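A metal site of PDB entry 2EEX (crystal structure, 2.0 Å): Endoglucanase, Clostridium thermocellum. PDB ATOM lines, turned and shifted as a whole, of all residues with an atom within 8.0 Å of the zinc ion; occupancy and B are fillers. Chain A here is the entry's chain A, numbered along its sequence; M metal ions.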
ATOM      1  N   GLU A  33     -34.525 -14.175 -23.593  1.00  0.00           N
ATOM      2  CA  GLU A  33     -34.967 -14.742 -22.325  1.00  0.00           C
ATOM      3  C   GLU A  33     -33.919 -15.781 -21.911  1.00  0.00           C
ATOM      4  O   GLU A  33     -33.762 -16.830 -22.546  1.00  0.00           O
ATOM      5  CB  GLU A  33     -36.360 -15.346 -22.490  1.00  0.00           C
ATOM      6  CG  GLU A  33     -37.378 -14.293 -22.970  1.00  0.00           C
ATOM      7  CD  GLU A  33     -38.796 -14.821 -23.140  1.00  0.00           C
ATOM      8  OE1 GLU A  33     -38.976 -15.855 -23.821  1.00  0.00           O
ATOM      9  OE2 GLU A  33     -39.725 -14.191 -22.601  1.00  0.00           O
ATOM     10  N   LEU A  34     -33.199 -15.458 -20.845  1.00  0.00           N
ATOM     11  CA  LEU A  34     -32.126 -16.313 -20.363  1.00  0.00           C
ATOM     12  C   LEU A  34     -32.434 -17.052 -19.082  1.00  0.00           C
ATOM     13  O   LEU A  34     -33.340 -16.699 -18.340  1.00  0.00           O
ATOM     14  CB  LEU A  34     -30.872 -15.481 -20.119  1.00  0.00           C
ATOM     15  CG  LEU A  34     -30.286 -14.683 -21.279  1.00  0.00           C
ATOM     16  CD1 LEU A  34     -29.093 -13.882 -20.768  1.00  0.00           C
ATOM     17  CD2 LEU A  34     -29.889 -15.626 -22.402  1.00  0.00           C
ATOM     18  N   ASP A  35     -31.631 -18.087 -18.825  1.00  0.00           N
ATOM     19  CA  ASP A  35     -31.738 -18.870 -17.604  1.00  0.00           C
ATOM     20  C   ASP A  35     -30.778 -18.176 -16.641  1.00  0.00           C
ATOM     21  O   ASP A  35     -29.765 -18.748 -16.229  1.00  0.00           O
ATOM     22  CB  ASP A  35     -31.273 -20.310 -17.842  1.00  0.00           C
ATOM     23  CG  ASP A  35     -32.071 -21.018 -18.920  1.00  0.00           C
ATOM     24  OD1 ASP A  35     -33.304 -20.964 -18.873  1.00  0.00           O
ATOM     25  OD2 ASP A  35     -31.451 -21.634 -19.811  1.00  0.00           O
ATOM     26  N   ALA A  36     -31.086 -16.922 -16.331  1.00  0.00           N
ATOM     27  CA  ALA A  36     -30.261 -16.130 -15.428  1.00  0.00           C
ATOM     28  C   ALA A  36     -31.062 -14.945 -14.913  1.00  0.00           C
ATOM     29  O   ALA A  36     -32.061 -14.548 -15.508  1.00  0.00           O
ATOM     30  CB  ALA A  36     -29.012 -15.633 -16.158  1.00  0.00           C
ATOM     31  N   GLY A 365     -20.258 -19.602 -25.324  1.00  0.00           N
ATOM     32  CA  GLY A 365     -21.325 -19.578 -24.341  1.00  0.00           C
ATOM     33  C   GLY A 365     -21.572 -20.849 -23.563  1.00  0.00           C
ATOM     34  O   GLY A 365     -22.039 -20.798 -22.418  1.00  0.00           O
ATOM     35  N   ASP A 394     -29.086 -16.724 -26.870  1.00  0.00           N
ATOM     36  CA  ASP A 394     -30.168 -17.457 -26.210  1.00  0.00           C
ATOM     37  C   ASP A 394     -29.762 -18.237 -24.956  1.00  0.00           C
ATOM     38  O   ASP A 394     -28.611 -18.223 -24.536  1.00  0.00           O
ATOM     39  CB  ASP A 394     -30.842 -18.419 -27.207  1.00  0.00           C
ATOM     40  CG  ASP A 394     -29.907 -19.479 -27.707  1.00  0.00           C
ATOM     41  OD1 ASP A 394     -29.108 -20.006 -26.899  1.00  0.00           O
ATOM     42  OD2 ASP A 394     -29.971 -19.808 -28.913  1.00  0.00           O
ATOM     43  N   ALA A 395     -30.742 -18.928 -24.384  1.00  0.00           N
ATOM     44  CA  ALA A 395     -30.549 -19.693 -23.159  1.00  0.00           C
ATOM     45  C   ALA A 395     -29.617 -20.900 -23.238  1.00  0.00           C
ATOM     46  O   ALA A 395     -29.347 -21.554 -22.219  1.00  0.00           O
ATOM     47  CB  ALA A 395     -31.917 -20.138 -22.624  1.00  0.00           C
ATOM     48  N   SER A 396     -29.110 -21.214 -24.424  1.00  0.00           N
ATOM     49  CA  SER A 396     -28.210 -22.364 -24.548  1.00  0.00           C
ATOM     50  C   SER A 396     -26.803 -22.007 -24.098  1.00  0.00           C
ATOM     51  O   SER A 396     -25.951 -22.878 -23.977  1.00  0.00           O
ATOM     52  CB  SER A 396     -28.179 -22.865 -25.999  1.00  0.00           C
ATOM     53  OG  SER A 396     -27.515 -21.955 -26.852  1.00  0.00           O
ATOM     54  N   ASN A 397     -26.558 -20.725 -23.849  1.00  0.00           N
ATOM     55  CA  ASN A 397     -25.243 -20.275 -23.393  1.00  0.00           C
ATOM     56  C   ASN A 397     -25.198 -20.391 -21.883  1.00  0.00           C
ATOM     57  O   ASN A 397     -25.174 -19.386 -21.173  1.00  0.00           O
ATOM     58  CB  ASN A 397     -25.029 -18.826 -23.840  1.00  0.00           C
ATOM     59  CG  ASN A 397     -25.003 -18.678 -25.345  1.00  0.00           C
ATOM     60  OD1 ASN A 397     -24.062 -19.145 -25.999  1.00  0.00           O
ATOM     61  ND2 ASN A 397     -26.032 -18.060 -25.914  1.00  0.00           N
ATOM     62  N   ASN A 398     -25.185 -21.628 -21.396  1.00  0.00           N
ATOM     63  CA  ASN A 398     -25.197 -21.889 -19.960  1.00  0.00           C
ATOM     64  C   ASN A 398     -24.050 -21.253 -19.184  1.00  0.00           C
ATOM     65  O   ASN A 398     -24.251 -20.775 -18.063  1.00  0.00           O
ATOM     66  CB  ASN A 398     -25.251 -23.406 -19.686  1.00  0.00           C
ATOM     67  CG  ASN A 398     -24.120 -24.179 -20.364  1.00  0.00           C
ATOM     68  OD1 ASN A 398     -23.922 -24.090 -21.571  1.00  0.00           O
ATOM     69  ND2 ASN A 398     -23.382 -24.963 -19.564  1.00  0.00           N
ATOM     70  N   TYR A 399     -22.853 -21.226 -19.757  1.00  0.00           N
ATOM     71  CA  TYR A 399     -21.725 -20.622 -19.063  1.00  0.00           C
ATOM     72  C   TYR A 399     -21.816 -19.107 -19.084  1.00  0.00           C
ATOM     73  O   TYR A 399     -21.391 -18.454 -18.129  1.00  0.00           O
ATOM     74  CB  TYR A 399     -20.406 -21.127 -19.652  1.00  0.00           C
ATOM     75  CG  TYR A 399     -19.934 -22.381 -18.966  1.00  0.00           C
ATOM     76  CD1 TYR A 399     -19.391 -22.329 -17.673  1.00  0.00           C
ATOM     77  CD2 TYR A 399     -20.082 -23.631 -19.573  1.00  0.00           C
ATOM     78  CE1 TYR A 399     -19.001 -23.502 -17.015  1.00  0.00           C
ATOM     79  CE2 TYR A 399     -19.696 -24.794 -18.916  1.00  0.00           C
ATOM     80  CZ  TYR A 399     -19.154 -24.725 -17.648  1.00  0.00           C
ATOM     81  OH  TYR A 399     -18.754 -25.882 -16.991  1.00  0.00           O
ATOM     82  N   THR A 400     -22.374 -18.537 -20.142  1.00  0.00           N
ATOM     83  CA  THR A 400     -22.537 -17.091 -20.204  1.00  0.00           C
ATOM     84  C   THR A 400     -23.503 -16.728 -19.073  1.00  0.00           C
ATOM     85  O   THR A 400     -23.283 -15.769 -18.344  1.00  0.00           O
ATOM     86  CB  THR A 400     -23.173 -16.630 -21.542  1.00  0.00           C
ATOM     87  OG1 THR A 400     -22.385 -17.097 -22.642  1.00  0.00           O
ATOM     88  CG2 THR A 400     -23.252 -15.093 -21.601  1.00  0.00           C
ATOM     89  N   GLU A 401     -24.567 -17.509 -18.934  1.00  0.00           N
ATOM     90  CA  GLU A 401     -25.554 -17.267 -17.892  1.00  0.00           C
ATOM     91  C   GLU A 401     -24.932 -17.398 -16.502  1.00  0.00           C
ATOM     92  O   GLU A 401     -25.312 -16.675 -15.584  1.00  0.00           O
ATOM     93  CB  GLU A 401     -26.736 -18.234 -18.073  1.00  0.00           C
ATOM     94  CG  GLU A 401     -27.407 -18.112 -19.457  1.00  0.00           C
ATOM     95  CD  GLU A 401     -28.468 -19.169 -19.701  1.00  0.00           C
ATOM     96  OE1 GLU A 401     -28.240 -20.344 -19.331  1.00  0.00           O
ATOM     97  OE2 GLU A 401     -29.524 -18.838 -20.281  1.00  0.00           O
ATOM     98  N   ALA A 402     -23.974 -18.317 -16.349  1.00  0.00           N
ATOM     99  CA  ALA A 402     -23.325 -18.483 -15.053  1.00  0.00           C
ATOM    100  C   ALA A 402     -22.546 -17.207 -14.740  1.00  0.00           C
ATOM    101  O   ALA A 402     -22.564 -16.707 -13.624  1.00  0.00           O
ATOM    102  CB  ALA A 402     -22.390 -19.689 -15.061  1.00  0.00           C
ATOM    103  N   SER A 484     -21.584 -25.514 -14.871  1.00  0.00           N
ATOM    104  CA  SER A 484     -21.898 -24.098 -14.998  1.00  0.00           C
ATOM    105  C   SER A 484     -22.795 -23.678 -13.829  1.00  0.00           C
ATOM    106  O   SER A 484     -23.106 -22.502 -13.666  1.00  0.00           O
ATOM    107  CB  SER A 484     -22.577 -23.810 -16.348  1.00  0.00           C
ATOM    108  OG  SER A 484     -23.691 -24.668 -16.578  1.00  0.00           O
HETATM  109 ZN    ZN M   1     -29.522 -21.548 -20.231  1.00  0.00          ZN
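Within 4 Å of the zinc ion: Asp 35, Ala 395 and Glu 401.
The zinc ion is bound by the side-chain carboxylate (OE1) of Glu 401 (2.0 Å), the side-chain carboxylate (OD2) of Asp 35 (2.0 Å) and the backbone carbonyl oxygen (O) of Ala 395 (2.0 Å). The zinc ion has three donor atoms within binding distance. Slightly farther from the zinc ion lies OE2 of Glu 401 (2.7 Å).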
